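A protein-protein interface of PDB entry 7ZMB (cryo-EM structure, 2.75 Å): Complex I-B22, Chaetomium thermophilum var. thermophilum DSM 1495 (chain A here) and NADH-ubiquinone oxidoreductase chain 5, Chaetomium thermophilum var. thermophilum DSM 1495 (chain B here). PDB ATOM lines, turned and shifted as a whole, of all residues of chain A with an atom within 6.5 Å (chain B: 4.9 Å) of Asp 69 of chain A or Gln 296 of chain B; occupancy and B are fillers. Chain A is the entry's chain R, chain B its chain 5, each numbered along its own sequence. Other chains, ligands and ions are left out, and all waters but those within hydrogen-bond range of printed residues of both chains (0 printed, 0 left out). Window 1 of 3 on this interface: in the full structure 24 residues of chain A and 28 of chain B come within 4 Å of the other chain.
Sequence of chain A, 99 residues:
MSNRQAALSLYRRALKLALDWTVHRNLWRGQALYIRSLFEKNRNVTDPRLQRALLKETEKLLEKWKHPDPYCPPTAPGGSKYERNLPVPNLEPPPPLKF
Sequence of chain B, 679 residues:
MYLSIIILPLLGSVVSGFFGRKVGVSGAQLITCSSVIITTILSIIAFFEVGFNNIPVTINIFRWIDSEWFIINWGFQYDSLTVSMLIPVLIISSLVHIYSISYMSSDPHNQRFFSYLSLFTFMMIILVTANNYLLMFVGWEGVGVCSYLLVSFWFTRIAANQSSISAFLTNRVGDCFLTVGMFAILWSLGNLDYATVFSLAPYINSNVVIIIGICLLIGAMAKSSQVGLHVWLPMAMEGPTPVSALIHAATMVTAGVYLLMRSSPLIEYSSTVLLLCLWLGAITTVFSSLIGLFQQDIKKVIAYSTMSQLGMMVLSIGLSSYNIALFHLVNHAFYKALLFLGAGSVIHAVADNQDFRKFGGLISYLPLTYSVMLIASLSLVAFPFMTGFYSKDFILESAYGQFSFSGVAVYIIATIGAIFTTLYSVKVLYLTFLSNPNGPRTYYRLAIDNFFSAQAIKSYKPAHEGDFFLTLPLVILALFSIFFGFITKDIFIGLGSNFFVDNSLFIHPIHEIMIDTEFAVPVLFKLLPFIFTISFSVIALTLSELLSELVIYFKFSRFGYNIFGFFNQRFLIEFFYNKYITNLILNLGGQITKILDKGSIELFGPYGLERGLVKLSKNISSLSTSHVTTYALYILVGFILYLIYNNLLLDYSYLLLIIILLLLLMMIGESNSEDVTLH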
ATOM      1  N   ASP A  20     -15.224  -7.272  20.725  1.00  0.00           N
ATOM      2  CA  ASP A  20     -14.782  -8.629  21.013  1.00  0.00           C
ATOM      3  C   ASP A  20     -15.397  -9.187  22.286  1.00  0.00           C
ATOM      4  O   ASP A  20     -15.362 -10.402  22.492  1.00  0.00           O
ATOM      5  CB  ASP A  20     -13.257  -8.683  21.096  1.00  0.00           C
ATOM      6  CG  ASP A  20     -12.620  -8.864  19.742  1.00  0.00           C
ATOM      7  OD1 ASP A  20     -13.371  -9.096  18.777  1.00  0.00           O
ATOM      8  OD2 ASP A  20     -11.381  -8.770  19.635  1.00  0.00           O
ATOM      9  N   LYS A  66      -9.571  -5.965  29.472  1.00  0.00           N
ATOM     10  CA  LYS A  66      -8.942  -6.693  28.379  1.00  0.00           C
ATOM     11  C   LYS A  66      -9.610  -8.048  28.180  1.00  0.00           C
ATOM     12  O   LYS A  66      -9.951  -8.742  29.139  1.00  0.00           O
ATOM     13  CB  LYS A  66      -7.444  -6.855  28.639  1.00  0.00           C
ATOM     14  CG  LYS A  66      -7.078  -7.760  29.805  1.00  0.00           C
ATOM     15  CD  LYS A  66      -5.569  -7.825  29.982  1.00  0.00           C
ATOM     16  CE  LYS A  66      -5.178  -8.688  31.167  1.00  0.00           C
ATOM     17  NZ  LYS A  66      -5.514 -10.115  30.950  1.00  0.00           N
ATOM     18  N   HIS A  67      -9.812  -8.408  26.921  1.00  0.00           N
ATOM     19  CA  HIS A  67     -10.539  -9.626  26.606  1.00  0.00           C
ATOM     20  C   HIS A  67      -9.671 -10.851  26.879  1.00  0.00           C
ATOM     21  O   HIS A  67      -8.450 -10.801  26.703  1.00  0.00           O
ATOM     22  CB  HIS A  67     -10.981  -9.619  25.147  1.00  0.00           C
ATOM     23  CG  HIS A  67     -12.176 -10.478  24.887  1.00  0.00           C
ATOM     24  ND1 HIS A  67     -12.084 -11.725  24.311  1.00  0.00           N
ATOM     25  CD2 HIS A  67     -13.486 -10.287  25.163  1.00  0.00           C
ATOM     26  CE1 HIS A  67     -13.288 -12.256  24.229  1.00  0.00           C
ATOM     27  NE2 HIS A  67     -14.156 -11.404  24.737  1.00  0.00           N
ATOM     28  N   PRO A  68     -10.269 -11.959  27.323  1.00  0.00           N
ATOM     29  CA  PRO A  68      -9.473 -13.185  27.489  1.00  0.00           C
ATOM     30  C   PRO A  68      -8.850 -13.657  26.190  1.00  0.00           C
ATOM     31  O   PRO A  68      -7.751 -14.225  26.200  1.00  0.00           O
ATOM     32  CB  PRO A  68     -10.490 -14.194  28.041  1.00  0.00           C
ATOM     33  CG  PRO A  68     -11.580 -13.369  28.621  1.00  0.00           C
ATOM     34  CD  PRO A  68     -11.648 -12.113  27.811  1.00  0.00           C
ATOM     35  N   ASP A  69      -9.525 -13.433  25.065  1.00  0.00           N
ATOM     36  CA  ASP A  69      -8.990 -13.767  23.749  1.00  0.00           C
ATOM     37  C   ASP A  69      -9.628 -12.862  22.703  1.00  0.00           C
ATOM     38  O   ASP A  69     -10.729 -13.149  22.208  1.00  0.00           O
ATOM     39  CB  ASP A  69      -9.209 -15.243  23.425  1.00  0.00           C
ATOM     40  CG  ASP A  69     -10.618 -15.705  23.733  1.00  0.00           C
ATOM     41  OD1 ASP A  69     -11.395 -14.906  24.298  1.00  0.00           O
ATOM     42  OD2 ASP A  69     -10.947 -16.868  23.422  1.00  0.00           O
ATOM     43  N   PRO A  70      -8.974 -11.762  22.344  1.00  0.00           N
ATOM     44  CA  PRO A  70      -9.522 -10.888  21.301  1.00  0.00           C
ATOM     45  C   PRO A  70      -9.535 -11.568  19.940  1.00  0.00           C
ATOM     46  O   PRO A  70      -8.794 -12.519  19.687  1.00  0.00           O
ATOM     47  CB  PRO A  70      -8.568  -9.687  21.311  1.00  0.00           C
ATOM     48  CG  PRO A  70      -7.941  -9.711  22.668  1.00  0.00           C
ATOM     49  CD  PRO A  70      -7.808 -11.164  23.013  1.00  0.00           C
ATOM     50  N   TYR A  71     -10.397 -11.067  19.062  1.00  0.00           N
ATOM     51  CA  TYR A  71     -10.457 -11.569  17.699  1.00  0.00           C
ATOM     52  C   TYR A  71      -9.236 -11.132  16.903  1.00  0.00           C
ATOM     53  O   TYR A  71      -8.756 -10.003  17.034  1.00  0.00           O
ATOM     54  CB  TYR A  71     -11.726 -11.076  17.002  1.00  0.00           C
ATOM     55  CG  TYR A  71     -11.738 -11.318  15.515  1.00  0.00           C
ATOM     56  CD1 TYR A  71     -12.239 -12.497  14.996  1.00  0.00           C
ATOM     57  CD2 TYR A  71     -11.242 -10.371  14.628  1.00  0.00           C
ATOM     58  CE1 TYR A  71     -12.244 -12.731  13.637  1.00  0.00           C
ATOM     59  CE2 TYR A  71     -11.243 -10.593  13.276  1.00  0.00           C
ATOM     60  CZ  TYR A  71     -11.747 -11.773  12.781  1.00  0.00           C
ATOM     61  OH  TYR A  71     -11.754 -12.001  11.425  1.00  0.00           O
ATOM     62  N   PHE B 294     -17.314 -21.118  26.616  1.00  0.00           N
ATOM     63  CA  PHE B 294     -16.715 -19.791  26.518  1.00  0.00           C
ATOM     64  C   PHE B 294     -15.612 -19.763  25.474  1.00  0.00           C
ATOM     65  O   PHE B 294     -14.581 -19.110  25.644  1.00  0.00           O
ATOM     66  CB  PHE B 294     -16.182 -19.360  27.879  1.00  0.00           C
ATOM     67  CG  PHE B 294     -17.131 -19.629  29.016  1.00  0.00           C
ATOM     68  CD1 PHE B 294     -17.199 -20.881  29.598  1.00  0.00           C
ATOM     69  CD2 PHE B 294     -17.962 -18.638  29.495  1.00  0.00           C
ATOM     70  CE1 PHE B 294     -18.077 -21.128  30.641  1.00  0.00           C
ATOM     71  CE2 PHE B 294     -18.835 -18.880  30.532  1.00  0.00           C
ATOM     72  CZ  PHE B 294     -18.894 -20.127  31.105  1.00  0.00           C
ATOM     73  N   GLN B 295     -15.828 -20.524  24.409  1.00  0.00           N
ATOM     74  CA  GLN B 295     -14.771 -20.682  23.405  1.00  0.00           C
ATOM     75  C   GLN B 295     -15.154 -19.985  22.112  1.00  0.00           C
ATOM     76  O   GLN B 295     -16.259 -20.220  21.628  1.00  0.00           O
ATOM     77  CB  GLN B 295     -14.300 -22.141  23.318  1.00  0.00           C
ATOM     78  CG  GLN B 295     -13.767 -22.712  24.620  1.00  0.00           C
ATOM     79  CD  GLN B 295     -12.627 -21.919  25.207  1.00  0.00           C
ATOM     80  OE1 GLN B 295     -11.780 -21.383  24.499  1.00  0.00           O
ATOM     81  NE2 GLN B 295     -12.597 -21.848  26.526  1.00  0.00           N
ATOM     82  N   GLN B 296     -14.257 -19.145  21.597  1.00  0.00           N
ATOM     83  CA  GLN B 296     -14.483 -18.388  20.375  1.00  0.00           C
ATOM     84  C   GLN B 296     -13.821 -19.044  19.169  1.00  0.00           C
ATOM     85  O   GLN B 296     -13.389 -18.354  18.242  1.00  0.00           O
ATOM     86  CB  GLN B 296     -13.995 -16.950  20.549  1.00  0.00           C
ATOM     87  CG  GLN B 296     -14.904 -16.096  21.429  1.00  0.00           C
ATOM     88  CD  GLN B 296     -14.899 -16.539  22.880  1.00  0.00           C
ATOM     89  OE1 GLN B 296     -13.855 -16.585  23.520  1.00  0.00           O
ATOM     90  NE2 GLN B 296     -16.068 -16.871  23.400  1.00  0.00           N
ATOM     91  N   ASP B 297     -13.719 -20.372  19.180  1.00  0.00           N
ATOM     92  CA  ASP B 297     -13.240 -21.145  18.045  1.00  0.00           C
ATOM     93  C   ASP B 297     -14.108 -22.381  17.928  1.00  0.00           C
ATOM     94  O   ASP B 297     -14.332 -23.078  18.920  1.00  0.00           O
ATOM     95  CB  ASP B 297     -11.765 -21.541  18.209  1.00  0.00           C
ATOM     96  CG  ASP B 297     -11.319 -22.593  17.197  1.00  0.00           C
ATOM     97  OD1 ASP B 297     -11.901 -22.668  16.095  1.00  0.00           O
ATOM     98  OD2 ASP B 297     -10.377 -23.351  17.505  1.00  0.00           O
ATOM     99  N   ILE B 298     -14.599 -22.653  16.720  1.00  0.00           N
ATOM    100  CA  ILE B 298     -15.461 -23.814  16.532  1.00  0.00           C
ATOM    101  C   ILE B 298     -14.660 -25.099  16.694  1.00  0.00           C
ATOM    102  O   ILE B 298     -15.133 -26.075  17.285  1.00  0.00           O
ATOM    103  CB  ILE B 298     -16.183 -23.739  15.172  1.00  0.00           C
ATOM    104  CG1 ILE B 298     -17.318 -24.764  15.113  1.00  0.00           C
ATOM    105  CG2 ILE B 298     -15.219 -23.915  14.010  1.00  0.00           C
ATOM    106  CD1 ILE B 298     -18.357 -24.456  14.063  1.00  0.00           C
ATOM    107  N   GLN B 354     -12.174 -19.096  12.029  1.00  0.00           N
ATOM    108  CA  GLN B 354     -12.606 -20.031  13.052  1.00  0.00           C
ATOM    109  C   GLN B 354     -13.302 -19.368  14.231  1.00  0.00           C
ATOM    110  O   GLN B 354     -13.708 -20.074  15.159  1.00  0.00           O
ATOM    111  CB  GLN B 354     -11.409 -20.851  13.558  1.00  0.00           C
ATOM    112  CG  GLN B 354     -10.706 -21.638  12.465  1.00  0.00           C
ATOM    113  CD  GLN B 354      -9.585 -22.505  12.993  1.00  0.00           C
ATOM    114  OE1 GLN B 354      -9.394 -22.622  14.202  1.00  0.00           O
ATOM    115  NE2 GLN B 354      -8.836 -23.120  12.086  1.00  0.00           N
ATOM    116  N   ASP B 355     -13.472 -18.051  14.218  1.00  0.00           N
ATOM    117  CA  ASP B 355     -14.054 -17.340  15.346  1.00  0.00           C
ATOM    118  C   ASP B 355     -15.565 -17.217  15.196  1.00  0.00           C
ATOM    119  O   ASP B 355     -16.075 -16.920  14.113  1.00  0.00           O
ATOM    120  CB  ASP B 355     -13.431 -15.951  15.485  1.00  0.00           C
ATOM    121  CG  ASP B 355     -13.541 -15.402  16.893  1.00  0.00           C
ATOM    122  OD1 ASP B 355     -14.535 -15.716  17.578  1.00  0.00           O
ATOM    123  OD2 ASP B 355     -12.631 -14.658  17.316  1.00  0.00           O
ATOM    124  N   PHE B 356     -16.278 -17.445  16.302  1.00  0.00           N
ATOM    125  CA  PHE B 356     -17.723 -17.260  16.312  1.00  0.00           C
ATOM    126  C   PHE B 356     -18.120 -15.796  16.210  1.00  0.00           C
ATOM    127  O   PHE B 356     -19.246 -15.501  15.797  1.00  0.00           O
ATOM    128  CB  PHE B 356     -18.326 -17.857  17.581  1.00  0.00           C
ATOM    129  CG  PHE B 356     -18.315 -19.352  17.614  1.00  0.00           C
ATOM    130  CD1 PHE B 356     -19.328 -20.076  17.012  1.00  0.00           C
ATOM    131  CD2 PHE B 356     -17.300 -20.035  18.255  1.00  0.00           C
ATOM    132  CE1 PHE B 356     -19.325 -21.454  17.044  1.00  0.00           C
ATOM    133  CE2 PHE B 356     -17.292 -21.411  18.292  1.00  0.00           C
ATOM    134  CZ  PHE B 356     -18.305 -22.121  17.684  1.00  0.00           C
ATOM    135  N   ARG B 357     -17.228 -14.877  16.584  1.00  0.00           N
ATOM    136  CA  ARG B 357     -17.562 -13.460  16.578  1.00  0.00           C
ATOM    137  C   ARG B 357     -17.829 -12.932  15.177  1.00  0.00           C
ATOM    138  O   ARG B 357     -18.454 -11.875  15.035  1.00  0.00           O
ATOM    139  CB  ARG B 357     -16.441 -12.659  17.233  1.00  0.00           C
ATOM    140  CG  ARG B 357     -16.108 -13.131  18.637  1.00  0.00           C
ATOM    141  CD  ARG B 357     -15.554 -12.008  19.491  1.00  0.00           C
ATOM    142  NE  ARG B 357     -14.751 -12.525  20.595  1.00  0.00           N
ATOM    143  CZ  ARG B 357     -13.488 -12.922  20.474  1.00  0.00           C
ATOM    144  NH1 ARG B 357     -12.829 -13.382  21.522  1.00  0.00           N
ATOM    145  NH2 ARG B 357     -12.889 -12.871  19.300  1.00  0.00           N
ATOM    146  N   LYS B 427     -24.885 -23.092  21.039  1.00  0.00           N
ATOM    147  CA  LYS B 427     -24.009 -21.955  20.777  1.00  0.00           C
ATOM    148  C   LYS B 427     -23.321 -22.094  19.425  1.00  0.00           C
ATOM    149  O   LYS B 427     -23.213 -21.120  18.671  1.00  0.00           O
ATOM    150  CB  LYS B 427     -22.974 -21.810  21.891  1.00  0.00           C
ATOM    151  CG  LYS B 427     -21.964 -20.698  21.650  1.00  0.00           C
ATOM    152  CD  LYS B 427     -20.728 -20.866  22.513  1.00  0.00           C
ATOM    153  CE  LYS B 427     -19.860 -19.617  22.480  1.00  0.00           C
ATOM    154  NZ  LYS B 427     -18.607 -19.781  23.261  1.00  0.00           N
ATOM    155  N   PHE B 564     -16.281 -15.450  33.314  1.00  0.00           N
ATOM    156  CA  PHE B 564     -16.082 -15.638  31.881  1.00  0.00           C
ATOM    157  C   PHE B 564     -14.614 -15.866  31.562  1.00  0.00           C
ATOM    158  O   PHE B 564     -14.271 -16.772  30.799  1.00  0.00           O
ATOM    159  CB  PHE B 564     -16.586 -14.429  31.103  1.00  0.00           C
ATOM    160  CG  PHE B 564     -16.811 -14.703  29.645  1.00  0.00           C
ATOM    161  CD1 PHE B 564     -17.894 -15.445  29.226  1.00  0.00           C
ATOM    162  CD2 PHE B 564     -15.884 -14.298  28.705  1.00  0.00           C
ATOM    163  CE1 PHE B 564     -18.089 -15.713  27.891  1.00  0.00           C
ATOM    164  CE2 PHE B 564     -16.067 -14.560  27.376  1.00  0.00           C
ATOM    165  CZ  PHE B 564     -17.169 -15.273  26.962  1.00  0.00           C
ATOM    166  N   ASN B 568     -12.921 -19.366  30.247  1.00  0.00           N
ATOM    167  CA  ASN B 568     -12.354 -19.225  28.911  1.00  0.00           C
ATOM    168  C   ASN B 568     -10.924 -19.726  28.871  1.00  0.00           C
ATOM    169  O   ASN B 568     -10.550 -20.502  27.983  1.00  0.00           O
ATOM    170  CB  ASN B 568     -12.407 -17.757  28.489  1.00  0.00           C
ATOM    171  CG  ASN B 568     -11.955 -17.535  27.075  1.00  0.00           C
ATOM    172  OD1 ASN B 568     -10.824 -17.846  26.715  1.00  0.00           O
ATOM    173  ND2 ASN B 568     -12.840 -16.988  26.258  1.00  0.00           N
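The side-chain carboxylate (OD1) of Asp 20 of chain A is in salt-bridge range of the guanidinium group (NH2) of Arg 357 of chain B (3.8 Å).
The guanidinium group (NH1) of Arg 357 of chain B lies close to a ring nitrogen (ND1) of His 67 of chain A, at 3.3 Å.
The side-chain carboxylate (OD2) of Asp 69 of chain A sits close to the side-chain amide oxygen (OE1) of Gln 296 of chain B (2.9 Å).
The guanidinium group (NH1) of Arg 357 of chain B lies within salt-bridge range of the side-chain carboxylate (OD1) of Asp 69 of chain A.
The side-chain amide nitrogen (ND2) of Asn 568 of chain B sits at hydrogen-bond distance from the side-chain carboxylate (OD1) of Asp 69 of chain A (3.2 Å).
N of Tyr 71 of chain A lies close to NH2 of Arg 357 of chain B.
O of Asp 20 of chain A sits at hydrogen-bond distance from NE2 of His 67 of chain A (2.7 Å).
OD2 of Asp 20 of chain A sits at hydrogen-bond distance from N of Tyr 71 of chain A, 2.6 Å away.
ND1 of His 67 of chain A is in hydrogen-bond range of O of Asp 69 of chain A (2.9 Å).
O of Phe 294 of chain B sits close to OE1 of Gln 296 of chain B, 3.4 Å away.
The backbone carbonyl oxygen (O) of Asn 568 of chain B lies within hydrogen-bond range of the side-chain amide nitrogen (NE2) of Gln 295 of chain B (2.9 Å).
ND2 of Asn 568 of chain B lies within hydrogen-bond range of OE1 of Gln 296 of chain B.
Among the printed residues, pairs that only touch across the chains: Tyr 71 of chain A with Asp 355 of chain B (3.2 Å), Pro 70 of chain A with Arg 357 of chain B (3.7 Å) and Pro 68 of chain A with Asn 568 of chain B (3.8 Å).
Of the printed residues of chain B, Asp 20 of chain A touches Arg 357.
Of the printed residues of chain B, Pro 68 of chain A touches Asn 568.
Asp 69 of chain A touches three residues of chain B.
Phe 294 of chain B touches none of the printed residues of chain A.
Of chain A, only Asp 69 comes within 4 Å of Gln 296 of chain B.
Asp 297 of chain B touches none of the printed residues of chain A.
Hydrophobic or aromatic side chains of chain A within 4 Å of the printed part of chain B: His 67, Pro 68 and Tyr 71.
Among the printed residues, 9 pairs touch across the chains.
Among the printed residues, Asp or Glu carboxylates within 4 Å of a Lys or Arg side-chain nitrogen of the other chain: Asp 20 of chain A with Arg 357 of chain B and Asp 69 of chain A with Arg 357 of chain B.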
